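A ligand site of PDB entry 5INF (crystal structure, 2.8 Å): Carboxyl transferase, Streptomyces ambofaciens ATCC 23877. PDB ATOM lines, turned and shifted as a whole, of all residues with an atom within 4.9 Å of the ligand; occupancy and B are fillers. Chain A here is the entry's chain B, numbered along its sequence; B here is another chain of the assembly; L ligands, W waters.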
ATOM      1  N   PHE A 113       3.550   2.632 -31.725  1.00  0.00           N
ATOM      2  CA  PHE A 113       3.862   1.578 -30.771  1.00  0.00           C
ATOM      3  C   PHE A 113       4.401   0.361 -31.470  1.00  0.00           C
ATOM      4  O   PHE A 113       5.075  -0.457 -30.833  1.00  0.00           O
ATOM      5  CB  PHE A 113       2.591   1.205 -29.973  1.00  0.00           C
ATOM      6  CG  PHE A 113       2.783   0.118 -28.937  1.00  0.00           C
ATOM      7  CD1 PHE A 113       3.340   0.410 -27.703  1.00  0.00           C
ATOM      8  CD2 PHE A 113       2.322  -1.164 -29.161  1.00  0.00           C
ATOM      9  CE1 PHE A 113       3.468  -0.586 -26.750  1.00  0.00           C
ATOM     10  CE2 PHE A 113       2.453  -2.141 -28.220  1.00  0.00           C
ATOM     11  CZ  PHE A 113       3.030  -1.856 -26.999  1.00  0.00           C
ATOM     12  N   LEU A 116       9.205  -1.053 -32.279  1.00  0.00           N
ATOM     13  CA  LEU A 116      10.010  -1.224 -31.082  1.00  0.00           C
ATOM     14  C   LEU A 116       9.278  -0.754 -29.826  1.00  0.00           C
ATOM     15  O   LEU A 116       9.863  -0.154 -28.923  1.00  0.00           O
ATOM     16  CB  LEU A 116      11.363  -0.521 -31.228  1.00  0.00           C
ATOM     17  CG  LEU A 116      12.262  -1.292 -32.205  1.00  0.00           C
ATOM     18  CD1 LEU A 116      13.346  -0.426 -32.849  1.00  0.00           C
ATOM     19  CD2 LEU A 116      12.875  -2.496 -31.474  1.00  0.00           C
ATOM     20  N   GLY A 117       7.975  -1.065 -29.762  1.00  0.00           N
ATOM     21  CA  GLY A 117       7.223  -0.810 -28.552  1.00  0.00           C
ATOM     22  C   GLY A 117       7.017   0.642 -28.221  1.00  0.00           C
ATOM     23  O   GLY A 117       6.742   0.962 -27.064  1.00  0.00           O
ATOM     24  N   SER A 119       9.371   2.836 -28.234  1.00  0.00           N
ATOM     25  CA  SER A 119      10.499   3.315 -27.436  1.00  0.00           C
ATOM     26  C   SER A 119      11.242   4.467 -28.120  1.00  0.00           C
ATOM     27  O   SER A 119      11.289   4.572 -29.341  1.00  0.00           O
ATOM     28  CB  SER A 119      11.475   2.178 -27.153  1.00  0.00           C
ATOM     29  OG  SER A 119      11.571   1.338 -28.283  1.00  0.00           O
ATOM     30  N   GLY A 149       6.651   2.161 -24.580  1.00  0.00           N
ATOM     31  CA  GLY A 149       7.329   1.599 -23.426  1.00  0.00           C
ATOM     32  C   GLY A 149       8.537   2.386 -22.951  1.00  0.00           C
ATOM     33  O   GLY A 149       9.451   1.826 -22.346  1.00  0.00           O
ATOM     34  N   GLY A 150       8.576   3.677 -23.251  1.00  0.00           N
ATOM     35  CA  GLY A 150       9.589   4.540 -22.687  1.00  0.00           C
ATOM     36  C   GLY A 150      10.908   4.564 -23.435  1.00  0.00           C
ATOM     37  O   GLY A 150      10.954   4.452 -24.664  1.00  0.00           O
ATOM     38  N   ALA A 151      11.991   4.712 -22.681  1.00  0.00           N
ATOM     39  CA  ALA A 151      13.323   4.803 -23.250  1.00  0.00           C
ATOM     40  C   ALA A 151      13.789   3.466 -23.829  1.00  0.00           C
ATOM     41  O   ALA A 151      13.519   2.400 -23.269  1.00  0.00           O
ATOM     42  CB  ALA A 151      14.298   5.281 -22.181  1.00  0.00           C
ATOM     43  N   ARG A 152      14.533   3.537 -24.936  1.00  0.00           N
ATOM     44  CA  ARG A 152      14.968   2.359 -25.660  1.00  0.00           C
ATOM     45  C   ARG A 152      16.245   1.794 -25.023  1.00  0.00           C
ATOM     46  O   ARG A 152      17.301   2.430 -25.072  1.00  0.00           O
ATOM     47  CB  ARG A 152      15.212   2.710 -27.121  1.00  0.00           C
ATOM     48  CG  ARG A 152      15.299   1.520 -28.012  1.00  0.00           C
ATOM     49  CD  ARG A 152      15.457   1.917 -29.434  1.00  0.00           C
ATOM     50  NE  ARG A 152      14.293   2.598 -29.955  1.00  0.00           N
ATOM     51  CZ  ARG A 152      14.257   3.184 -31.143  1.00  0.00           C
ATOM     52  NH1 ARG A 152      15.329   3.168 -31.933  1.00  0.00           N
ATOM     53  NH2 ARG A 152      13.142   3.814 -31.548  1.00  0.00           N
ATOM     54  N   ILE A 153      16.136   0.583 -24.467  1.00  0.00           N
ATOM     55  CA  ILE A 153      17.224   0.025 -23.665  1.00  0.00           C
ATOM     56  C   ILE A 153      18.473  -0.185 -24.498  1.00  0.00           C
ATOM     57  O   ILE A 153      19.596   0.026 -24.016  1.00  0.00           O
ATOM     58  CB  ILE A 153      16.754  -1.285 -23.025  1.00  0.00           C
ATOM     59  CG1 ILE A 153      15.516  -1.004 -22.197  1.00  0.00           C
ATOM     60  CG2 ILE A 153      17.865  -1.880 -22.183  1.00  0.00           C
ATOM     61  CD1 ILE A 153      14.389  -1.935 -22.443  1.00  0.00           C
ATOM     62  N   GLN A 154      18.317  -0.638 -25.739  1.00  0.00           N
ATOM     63  CA  GLN A 154      19.465  -0.975 -26.553  1.00  0.00           C
ATOM     64  C   GLN A 154      20.295   0.246 -26.897  1.00  0.00           C
ATOM     65  O   GLN A 154      21.473   0.110 -27.244  1.00  0.00           O
ATOM     66  CB  GLN A 154      19.027  -1.707 -27.815  1.00  0.00           C
ATOM     67  CG  GLN A 154      17.998  -0.950 -28.612  1.00  0.00           C
ATOM     68  CD  GLN A 154      16.682  -1.690 -28.749  1.00  0.00           C
ATOM     69  OE1 GLN A 154      16.042  -2.044 -27.757  1.00  0.00           O
ATOM     70  NE2 GLN A 154      16.231  -1.875 -29.989  1.00  0.00           N
ATOM     71  N   SER A 159      19.130   7.125 -24.866  1.00  0.00           N
ATOM     72  CA  SER A 159      17.685   7.294 -24.776  1.00  0.00           C
ATOM     73  C   SER A 159      17.265   7.919 -23.451  1.00  0.00           C
ATOM     74  O   SER A 159      16.280   8.660 -23.417  1.00  0.00           O
ATOM     75  CB  SER A 159      16.975   5.967 -25.011  1.00  0.00           C
ATOM     76  OG  SER A 159      17.436   5.021 -24.092  1.00  0.00           O
ATOM     77  N   ILE A 160      17.997   7.702 -22.359  1.00  0.00           N
ATOM     78  CA  ILE A 160      17.726   8.480 -21.148  1.00  0.00           C
ATOM     79  C   ILE A 160      17.993   9.962 -21.402  1.00  0.00           C
ATOM     80  O   ILE A 160      17.195  10.835 -21.037  1.00  0.00           O
ATOM     81  CB  ILE A 160      18.553   7.980 -19.951  1.00  0.00           C
ATOM     82  CG1 ILE A 160      18.268   6.525 -19.661  1.00  0.00           C
ATOM     83  CG2 ILE A 160      18.228   8.802 -18.744  1.00  0.00           C
ATOM     84  CD1 ILE A 160      19.172   6.019 -18.608  1.00  0.00           C
ATOM     85  N   TYR A 163      15.003  11.547 -23.443  1.00  0.00           N
ATOM     86  CA  TYR A 163      13.841  11.735 -22.589  1.00  0.00           C
ATOM     87  C   TYR A 163      14.080  12.833 -21.570  1.00  0.00           C
ATOM     88  O   TYR A 163      13.147  13.544 -21.199  1.00  0.00           O
ATOM     89  CB  TYR A 163      13.479  10.434 -21.849  1.00  0.00           C
ATOM     90  CG  TYR A 163      12.223   9.785 -22.390  1.00  0.00           C
ATOM     91  CD1 TYR A 163      11.004  10.447 -22.372  1.00  0.00           C
ATOM     92  CD2 TYR A 163      12.263   8.516 -22.938  1.00  0.00           C
ATOM     93  CE1 TYR A 163       9.860   9.875 -22.890  1.00  0.00           C
ATOM     94  CE2 TYR A 163      11.117   7.930 -23.452  1.00  0.00           C
ATOM     95  CZ  TYR A 163       9.923   8.629 -23.422  1.00  0.00           C
ATOM     96  OH  TYR A 163       8.779   8.057 -23.939  1.00  0.00           O
ATOM     97  N   THR A 164      15.311  12.955 -21.079  1.00  0.00           N
ATOM     98  CA  THR A 164      15.632  14.030 -20.157  1.00  0.00           C
ATOM     99  C   THR A 164      15.481  15.365 -20.849  1.00  0.00           C
ATOM    100  O   THR A 164      14.947  16.308 -20.260  1.00  0.00           O
ATOM    101  CB  THR A 164      17.045  13.883 -19.623  1.00  0.00           C
ATOM    102  OG1 THR A 164      17.188  12.621 -18.995  1.00  0.00           O
ATOM    103  CG2 THR A 164      17.328  14.939 -18.600  1.00  0.00           C
ATOM    104  N   GLY A 167      11.832  16.199 -21.119  1.00  0.00           N
ATOM    105  CA  GLY A 167      11.334  16.689 -19.846  1.00  0.00           C
ATOM    106  C   GLY A 167      11.791  18.099 -19.561  1.00  0.00           C
ATOM    107  O   GLY A 167      11.030  18.918 -19.071  1.00  0.00           O
ATOM    108  N   ASN A 170       9.478  20.258 -21.049  1.00  0.00           N
ATOM    109  CA  ASN A 170       8.232  20.319 -20.301  1.00  0.00           C
ATOM    110  C   ASN A 170       8.304  21.344 -19.183  1.00  0.00           C
ATOM    111  O   ASN A 170       7.364  22.103 -18.971  1.00  0.00           O
ATOM    112  CB  ASN A 170       7.906  18.951 -19.711  1.00  0.00           C
ATOM    113  CG  ASN A 170       7.598  17.935 -20.737  1.00  0.00           C
ATOM    114  OD1 ASN A 170       8.068  16.808 -20.663  1.00  0.00           O
ATOM    115  ND2 ASN A 170       6.795  18.315 -21.734  1.00  0.00           N
ATOM    116  N   ALA A 188       5.096   3.255 -19.872  1.00  0.00           N
ATOM    117  CA  ALA A 188       5.974   3.090 -18.720  1.00  0.00           C
ATOM    118  C   ALA A 188       7.132   4.056 -18.856  1.00  0.00           C
ATOM    119  O   ALA A 188       7.301   4.711 -19.886  1.00  0.00           O
ATOM    120  CB  ALA A 188       6.510   1.662 -18.624  1.00  0.00           C
ATOM    121  N   GLY A 189       7.919   4.140 -17.793  1.00  0.00           N
ATOM    122  CA  GLY A 189       9.131   4.965 -17.760  1.00  0.00           C
ATOM    123  C   GLY A 189       8.903   6.376 -18.267  1.00  0.00           C
ATOM    124  O   GLY A 189       7.945   7.059 -17.903  1.00  0.00           O
ATOM    125  N   GLY A 190       9.805   6.833 -19.133  1.00  0.00           N
ATOM    126  CA  GLY A 190       9.751   8.214 -19.566  1.00  0.00           C
ATOM    127  C   GLY A 190       8.426   8.590 -20.189  1.00  0.00           C
ATOM    128  O   GLY A 190       8.052   9.766 -20.188  1.00  0.00           O
ATOM    129  N   TYR A 193       6.538   9.731 -17.257  1.00  0.00           N
ATOM    130  CA  TYR A 193       7.199  10.850 -16.580  1.00  0.00           C
ATOM    131  C   TYR A 193       6.997  12.168 -17.311  1.00  0.00           C
ATOM    132  O   TYR A 193       6.737  13.193 -16.699  1.00  0.00           O
ATOM    133  CB  TYR A 193       8.692  10.590 -16.425  1.00  0.00           C
ATOM    134  CG  TYR A 193       9.086   9.464 -15.503  1.00  0.00           C
ATOM    135  CD1 TYR A 193       8.312   9.122 -14.404  1.00  0.00           C
ATOM    136  CD2 TYR A 193      10.232   8.722 -15.748  1.00  0.00           C
ATOM    137  CE1 TYR A 193       8.670   8.074 -13.569  1.00  0.00           C
ATOM    138  CE2 TYR A 193      10.601   7.678 -14.921  1.00  0.00           C
ATOM    139  CZ  TYR A 193       9.821   7.356 -13.835  1.00  0.00           C
ATOM    140  OH  TYR A 193      10.190   6.304 -13.035  1.00  0.00           O
ATOM    141  N   SER A 194       7.185  12.174 -18.629  1.00  0.00           N
ATOM    142  CA  SER A 194       6.963  13.421 -19.356  1.00  0.00           C
ATOM    143  C   SER A 194       5.499  13.876 -19.292  1.00  0.00           C
ATOM    144  O   SER A 194       5.252  15.053 -18.961  1.00  0.00           O
ATOM    145  CB  SER A 194       7.461  13.236 -20.791  1.00  0.00           C
ATOM    146  OG  SER A 194       7.278  14.387 -21.581  1.00  0.00           O
ATOM    147  N   LEU A 197       4.648  15.913 -16.273  1.00  0.00           N
ATOM    148  CA  LEU A 197       5.006  17.325 -16.288  1.00  0.00           C
ATOM    149  C   LEU A 197       4.082  18.157 -17.157  1.00  0.00           C
ATOM    150  O   LEU A 197       4.020  19.373 -16.990  1.00  0.00           O
ATOM    151  CB  LEU A 197       6.449  17.503 -16.770  1.00  0.00           C
ATOM    152  CG  LEU A 197       7.498  16.838 -15.895  1.00  0.00           C
ATOM    153  CD1 LEU A 197       8.811  16.609 -16.650  1.00  0.00           C
ATOM    154  CD2 LEU A 197       7.726  17.651 -14.647  1.00  0.00           C
ATOM    155  N   VAL A 212       5.417   3.229 -13.644  1.00  0.00           N
ATOM    156  CA  VAL A 212       6.842   3.513 -13.825  1.00  0.00           C
ATOM    157  C   VAL A 212       7.558   2.297 -14.385  1.00  0.00           C
ATOM    158  O   VAL A 212       8.490   2.429 -15.178  1.00  0.00           O
ATOM    159  CB  VAL A 212       7.479   4.024 -12.525  1.00  0.00           C
ATOM    160  CG1 VAL A 212       6.615   5.137 -11.938  1.00  0.00           C
ATOM    161  CG2 VAL A 212       7.685   2.882 -11.518  1.00  0.00           C
ATOM    162  N   THR A 213       7.123   1.089 -14.007  1.00  0.00           N
ATOM    163  CA  THR A 213       7.526  -0.102 -14.742  1.00  0.00           C
ATOM    164  C   THR A 213       6.411  -1.130 -14.648  1.00  0.00           C
ATOM    165  O   THR A 213       5.605  -1.117 -13.710  1.00  0.00           O
ATOM    166  CB  THR A 213       8.858  -0.677 -14.256  1.00  0.00           C
ATOM    167  OG1 THR A 213       9.322  -1.654 -15.209  1.00  0.00           O
ATOM    168  CG2 THR A 213       8.718  -1.299 -12.833  1.00  0.00           C
ATOM    169  N   GLY A 214       6.392  -2.031 -15.630  1.00  0.00           N
ATOM    170  CA  GLY A 214       5.290  -2.926 -15.864  1.00  0.00           C
ATOM    171  C   GLY A 214       5.176  -4.037 -14.845  1.00  0.00           C
ATOM    172  O   GLY A 214       6.096  -4.301 -14.069  1.00  0.00           O
ATOM    173  N   GLU A 216       5.243  -7.256 -15.116  1.00  0.00           N
ATOM    174  CA  GLU A 216       6.169  -8.371 -15.255  1.00  0.00           C
ATOM    175  C   GLU A 216       7.491  -8.054 -14.560  1.00  0.00           C
ATOM    176  O   GLU A 216       8.115  -8.943 -13.970  1.00  0.00           O
ATOM    177  CB  GLU A 216       6.373  -8.715 -16.736  1.00  0.00           C
ATOM    178  CG  GLU A 216       7.230  -7.716 -17.541  1.00  0.00           C
ATOM    179  CD  GLU A 216       6.416  -6.631 -18.227  1.00  0.00           C
ATOM    180  OE1 GLU A 216       5.713  -5.842 -17.539  1.00  0.00           O
ATOM    181  OE2 GLU A 216       6.489  -6.556 -19.461  1.00  0.00           O
ATOM    182  N   VAL A 217       7.910  -6.788 -14.617  1.00  0.00           N
ATOM    183  CA  VAL A 217       9.127  -6.364 -13.943  1.00  0.00           C
ATOM    184  C   VAL A 217       8.885  -6.214 -12.462  1.00  0.00           C
ATOM    185  O   VAL A 217       9.755  -6.533 -11.643  1.00  0.00           O
ATOM    186  CB  VAL A 217       9.648  -5.061 -14.581  1.00  0.00           C
ATOM    187  CG1 VAL A 217      11.040  -4.732 -14.078  1.00  0.00           C
ATOM    188  CG2 VAL A 217       9.618  -5.151 -16.108  1.00  0.00           C
ATOM    189  N   ILE B 402       8.117  12.751  -9.904  1.00  0.00           N
ATOM    190  CA  ILE B 402       8.672  13.627 -10.933  1.00  0.00           C
ATOM    191  C   ILE B 402       8.907  15.036 -10.421  1.00  0.00           C
ATOM    192  O   ILE B 402       9.631  15.794 -11.067  1.00  0.00           O
ATOM    193  CB  ILE B 402       7.754  13.636 -12.167  1.00  0.00           C
ATOM    194  CG1 ILE B 402       8.557  13.925 -13.420  1.00  0.00           C
ATOM    195  CG2 ILE B 402       6.705  14.718 -12.085  1.00  0.00           C
ATOM    196  CD1 ILE B 402       9.408  12.776 -13.843  1.00  0.00           C
ATOM    197  N   PHE B 405      12.461  15.821 -10.685  1.00  0.00           N
ATOM    198  CA  PHE B 405      12.843  16.248 -12.026  1.00  0.00           C
ATOM    199  C   PHE B 405      12.594  17.749 -12.207  1.00  0.00           C
ATOM    200  O   PHE B 405      13.534  18.497 -12.483  1.00  0.00           O
ATOM    201  CB  PHE B 405      12.101  15.436 -13.071  1.00  0.00           C
ATOM    202  CG  PHE B 405      12.631  15.627 -14.437  1.00  0.00           C
ATOM    203  CD1 PHE B 405      12.319  16.751 -15.154  1.00  0.00           C
ATOM    204  CD2 PHE B 405      13.449  14.684 -15.026  1.00  0.00           C
ATOM    205  CE1 PHE B 405      12.838  16.956 -16.444  1.00  0.00           C
ATOM    206  CE2 PHE B 405      13.967  14.877 -16.334  1.00  0.00           C
ATOM    207  CZ  PHE B 405      13.655  16.005 -17.037  1.00  0.00           C
ATOM    208  N   GLY B 425      18.356   4.399 -15.407  1.00  0.00           N
ATOM    209  CA  GLY B 425      17.046   4.883 -15.782  1.00  0.00           C
ATOM    210  C   GLY B 425      16.716   6.243 -15.230  1.00  0.00           C
ATOM    211  O   GLY B 425      17.546   7.162 -15.179  1.00  0.00           O
ATOM    212  N   GLY B 426      15.454   6.386 -14.796  1.00  0.00           N
ATOM    213  CA  GLY B 426      14.991   7.655 -14.279  1.00  0.00           C
ATOM    214  C   GLY B 426      15.803   8.149 -13.105  1.00  0.00           C
ATOM    215  O   GLY B 426      15.908   9.355 -12.877  1.00  0.00           O
ATOM    216  N   ALA B 429      18.700  10.008 -14.702  1.00  0.00           N
ATOM    217  CA  ALA B 429      18.206  11.240 -15.288  1.00  0.00           C
ATOM    218  C   ALA B 429      17.961  12.287 -14.220  1.00  0.00           C
ATOM    219  O   ALA B 429      18.348  13.445 -14.366  1.00  0.00           O
ATOM    220  CB  ALA B 429      16.914  10.964 -16.060  1.00  0.00           C
ATOM    221  N   VAL B 451      20.081   1.986 -18.880  1.00  0.00           N
ATOM    222  CA  VAL B 451      18.638   2.123 -18.716  1.00  0.00           C
ATOM    223  C   VAL B 451      18.091   1.176 -17.646  1.00  0.00           C
ATOM    224  O   VAL B 451      17.111   1.516 -16.971  1.00  0.00           O
ATOM    225  CB  VAL B 451      17.978   1.923 -20.084  1.00  0.00           C
ATOM    226  CG1 VAL B 451      16.540   2.327 -20.079  1.00  0.00           C
ATOM    227  CG2 VAL B 451      18.704   2.719 -21.113  1.00  0.00           C
ATOM    228  N   MET B 452      18.668  -0.018 -17.481  1.00  0.00           N
ATOM    229  CA  MET B 452      18.198  -1.016 -16.500  1.00  0.00           C
ATOM    230  C   MET B 452      19.390  -1.883 -16.105  1.00  0.00           C
ATOM    231  O   MET B 452      20.540  -1.458 -16.250  1.00  0.00           O
ATOM    232  CB  MET B 452      17.068  -1.857 -17.077  1.00  0.00           C
ATOM    233  CG  MET B 452      15.745  -1.220 -17.075  1.00  0.00           C
ATOM    234  SD  MET B 452      14.601  -2.300 -17.918  1.00  0.00           S
ATOM    235  CE  MET B 452      15.615  -2.866 -19.228  1.00  0.00           C
ATOM    236  N   PRO B 459      13.002  -7.578 -21.327  1.00  0.00           N
ATOM    237  CA  PRO B 459      12.209  -6.928 -22.329  1.00  0.00           C
ATOM    238  C   PRO B 459      12.970  -7.006 -23.623  1.00  0.00           C
ATOM    239  O   PRO B 459      12.559  -6.347 -24.561  1.00  0.00           O
ATOM    240  CB  PRO B 459      12.091  -5.506 -21.808  1.00  0.00           C
ATOM    241  CG  PRO B 459      12.004  -5.684 -20.356  1.00  0.00           C
ATOM    242  CD  PRO B 459      13.018  -6.770 -20.086  1.00  0.00           C
ATOM    243  N   ILE B 460      14.057  -7.762 -23.711  1.00  0.00           N
ATOM    244  CA  ILE B 460      14.834  -7.639 -24.934  1.00  0.00           C
ATOM    245  C   ILE B 460      15.047  -8.903 -25.724  1.00  0.00           C
ATOM    246  O   ILE B 460      15.212  -8.815 -26.940  1.00  0.00           O
ATOM    247  CB  ILE B 460      16.147  -6.935 -24.598  1.00  0.00           C
ATOM    248  CG1 ILE B 460      15.978  -5.420 -24.482  1.00  0.00           C
ATOM    249  CG2 ILE B 460      17.206  -7.081 -25.778  1.00  0.00           C
ATOM    250  CD1 ILE B 460      15.436  -4.719 -25.760  1.00  0.00           C
ATOM    251  N   HIS B 462      12.906 -12.054 -25.676  1.00  0.00           N
ATOM    252  CA  HIS B 462      11.804 -12.883 -25.211  1.00  0.00           C
ATOM    253  C   HIS B 462      11.822 -14.264 -25.860  1.00  0.00           C
ATOM    254  O   HIS B 462      12.574 -14.513 -26.801  1.00  0.00           O
ATOM    255  CB  HIS B 462      10.461 -12.188 -25.480  1.00  0.00           C
ATOM    256  CG  HIS B 462       9.924 -11.437 -24.306  1.00  0.00           C
ATOM    257  ND1 HIS B 462       9.197 -12.038 -23.292  1.00  0.00           N
ATOM    258  CD2 HIS B 462       9.972 -10.116 -23.984  1.00  0.00           C
ATOM    259  CE1 HIS B 462       8.847 -11.132 -22.400  1.00  0.00           C
ATOM    260  NE2 HIS B 462       9.299  -9.957 -22.806  1.00  0.00           N
HETATM  261  C1  LIG L   1      13.463  -1.381 -26.171  1.00  0.00           C
HETATM  262  C2  LIG L   1      11.336  -2.323 -26.015  1.00  0.00           C
HETATM  263  C3  LIG L   1      11.043  -1.467 -24.970  1.00  0.00           C
HETATM  264  C4  LIG L   1      11.998  -0.554 -24.537  1.00  0.00           C
HETATM  265  C5  LIG L   1       9.300  -2.708 -25.355  1.00  0.00           C
HETATM  266  N1  LIG L   1      10.233  -3.091 -26.246  1.00  0.00           N
HETATM  267  N2  LIG L   1       9.775  -1.723 -24.570  1.00  0.00           N
HETATM  268  N3  LIG L   1      12.543  -2.265 -26.619  1.00  0.00           N
HETATM  269  N4  LIG L   1      13.200  -0.536 -25.152  1.00  0.00           N
HETATM  270  N5  LIG L   1      11.675   0.313 -23.466  1.00  0.00           N
HETATM  271  C6  LIG L   1      10.108  -4.093 -27.253  1.00  0.00           C
HETATM  272  C7  LIG L   1       9.937  -5.284 -26.820  1.00  0.00           C
HETATM  273  O1  LIG L   1      11.247  -5.977 -26.705  1.00  0.00           O
HETATM  274  C8  LIG L   1       8.974  -5.953 -27.904  1.00  0.00           C
HETATM  275  O2  LIG L   1       9.578  -6.174 -29.079  1.00  0.00           O
HETATM  276  C9  LIG L   1       7.978  -4.800 -28.111  1.00  0.00           C
HETATM  277  O3  LIG L   1       8.796  -3.816 -28.267  1.00  0.00           O
HETATM  278  C10 LIG L   1       7.289  -4.491 -26.768  1.00  0.00           C
HETATM  279  O4  LIG L   1       5.950  -4.897 -26.635  1.00  0.00           O
HETATM  280  P1  LIG L   1       5.621  -5.190 -25.117  1.00  0.00           P
HETATM  281  O5  LIG L   1       4.982  -6.565 -25.046  1.00  0.00           O
HETATM  282  O6  LIG L   1       4.658  -4.150 -24.584  1.00  0.00           O
HETATM  283  O7  LIG L   1       7.032  -5.067 -24.348  1.00  0.00           O
HETATM  284  P2  LIG L   1       7.279  -5.211 -22.765  1.00  0.00           P
HETATM  285  O8  LIG L   1       6.101  -5.883 -22.092  1.00  0.00           O
HETATM  286  O9  LIG L   1       8.551  -5.992 -22.531  1.00  0.00           O
HETATM  287  O10 LIG L   1       7.448  -3.782 -22.076  1.00  0.00           O
HETATM  288  C11 LIG L   1       7.645  -3.763 -20.661  1.00  0.00           C
HETATM  289  C12 LIG L   1       7.869  -2.307 -20.228  1.00  0.00           C
HETATM  290  C13 LIG L   1       9.310  -1.967 -20.606  1.00  0.00           C
HETATM  291  C14 LIG L   1       6.909  -1.405 -20.968  1.00  0.00           C
HETATM  292  C15 LIG L   1       7.655  -2.162 -18.723  1.00  0.00           C
HETATM  293  O11 LIG L   1       9.315  -1.476 -21.900  1.00  0.00           O
HETATM  294  C16 LIG L   1       9.936  -0.942 -19.662  1.00  0.00           C
HETATM  295  O12 LIG L   1      10.551  -1.298 -18.688  1.00  0.00           O
HETATM  296  N6  LIG L   1       9.822   0.475 -19.966  1.00  0.00           N
HETATM  297  C17 LIG L   1      10.462   1.435 -19.093  1.00  0.00           C
HETATM  298  C18 LIG L   1      11.679   2.004 -19.855  1.00  0.00           C
HETATM  299  C19 LIG L   1      11.974   3.409 -19.349  1.00  0.00           C
HETATM  300  O13 LIG L   1      11.289   4.352 -19.741  1.00  0.00           O
HETATM  301  N7  LIG L   1      13.069   3.485 -18.415  1.00  0.00           N
HETATM  302  C20 LIG L   1      13.592   4.636 -17.724  1.00  0.00           C
HETATM  303  C21 LIG L   1      13.141   5.960 -18.275  1.00  0.00           C
HETATM  304  S1  LIG L   1      14.249   7.207 -17.689  1.00  0.00           S
HETATM  305  P3  LIG L   1      10.118  -7.605 -29.575  1.00  0.00           P
HETATM  306  O14 LIG L   1       9.729  -7.771 -31.018  1.00  0.00           O
HETATM  307  O15 LIG L   1       9.515  -8.731 -28.766  1.00  0.00           O
HETATM  308  O16 LIG L   1      11.625  -7.638 -29.452  1.00  0.00           O
HETATM  309  C22 LIG L   1      13.821   8.658 -18.581  1.00  0.00           C
HETATM  310  C23 LIG L   1      13.820  10.026 -17.913  1.00  0.00           C
HETATM  311  C24 LIG L   1      12.648  10.849 -18.435  1.00  0.00           C
HETATM  312  O17 LIG L   1      13.506   8.525 -19.739  1.00  0.00           O
HETATM  313  C25 LIG L   1      12.605  12.208 -17.743  1.00  0.00           C
HETATM  314  C26 LIG L   1      11.164  12.661 -17.502  1.00  0.00           C
HETATM  315  C27 LIG L   1      10.656  13.577 -18.618  1.00  0.00           C
HETATM  316  O   HOH W   1       3.277  -5.839 -27.696  1.00  0.00           O
HETATM  317  O   HOH W   2       2.487  -4.966 -23.423  1.00  0.00           O
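N of Gly 190 lies within hydrogen-bond range of O13 of the ligand, at 3.0 Å. O13 of the ligand sits at hydrogen-bond distance from N of Ala 151. O3 of the ligand lies within hydrogen-bond range of N of Gly 117 (3.2 Å). The backbone carbonyl oxygen of Pro 459 of chain B lies within hydrogen-bond range of an oxygen (O1) of the ligand (2.5 Å). N of Ile 153 lies within hydrogen-bond range of N4 of the ligand (3.2 Å). O of Ala 151 lies within hydrogen-bond range of N5 of the ligand. The backbone carbonyl oxygen (O) of Gly 149 sits at hydrogen-bond distance from a nitrogen (N6) of the ligand, at 2.8 Å. N of Gly 426 of chain B sits close to S1 of the ligand (3.2 Å). The side-chain carboxylate of Glu 216 lies close to an oxygen (O8) of the ligand (2.7 Å).
The backbone NH (N) of Gly 189 is in hydrogen-bond range of the backbone carbonyl oxygen (O) of Val 212, at 3.2 Å. The guanidinium group of Arg 152 sits at hydrogen-bond distance from the backbone carbonyl oxygen of Ser 119 (3.0 Å). The backbone carbonyl oxygen (O) of Arg 152 sits at hydrogen-bond distance from the side-chain hydroxyl (OG) of Ser 159, at 2.8 Å. The side-chain amide oxygen (OD1) of Asn 170 sits at hydrogen-bond distance from the side-chain hydroxyl (OG) of Ser 194. The backbone carbonyl oxygen of Gly 117 lies within hydrogen-bond range of the backbone NH of Gly 149 (2.8 Å).
Phe 113 touches the ligand. C of Leu 116 touches O3 of the ligand, 3.5 Å away. Ser 119 touches the ligand (CB to N4, 3.8 Å). CA of Gly 150 touches O13 of the ligand, 3.4 Å away. CA of Arg 152 touches N4 of the ligand (3.4 Å). OE1 of Gln 154 touches C1 of the ligand (3.1 Å). Tyr 163 touches the ligand (CB to O17, 2.8 Å). Gly 167 touches the ligand. CB of Ala 188 touches N6 of the ligand (3.8 Å). CA of Gly 189 touches O13 of the ligand (3.0 Å). CB of Tyr 193 touches C26 of the ligand (3.4 Å). Ser 194 touches the ligand. OG1 of Thr 213 touches O12 of the ligand, 3.7 Å away. Gly 214 touches the ligand (N to C15, 3.3 Å). CE2 of Phe 405 of chain B touches C25 of the ligand, at 3.3 Å. Gly 425 of chain B touches the ligand. CB of Ala 429 of chain B touches C23 of the ligand (3.7 Å). Ile 460 of chain B touches the ligand (CD1 to N3, 3.9 Å). Of the 37 residues printed, 26 come within 4 Å of the ligand. Along chain A the residues within 4 Å of the ligand span positions 113 to 216. The nearest printed residue that does not touch the ligand is Val 451 of chain B (4.02 Å).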
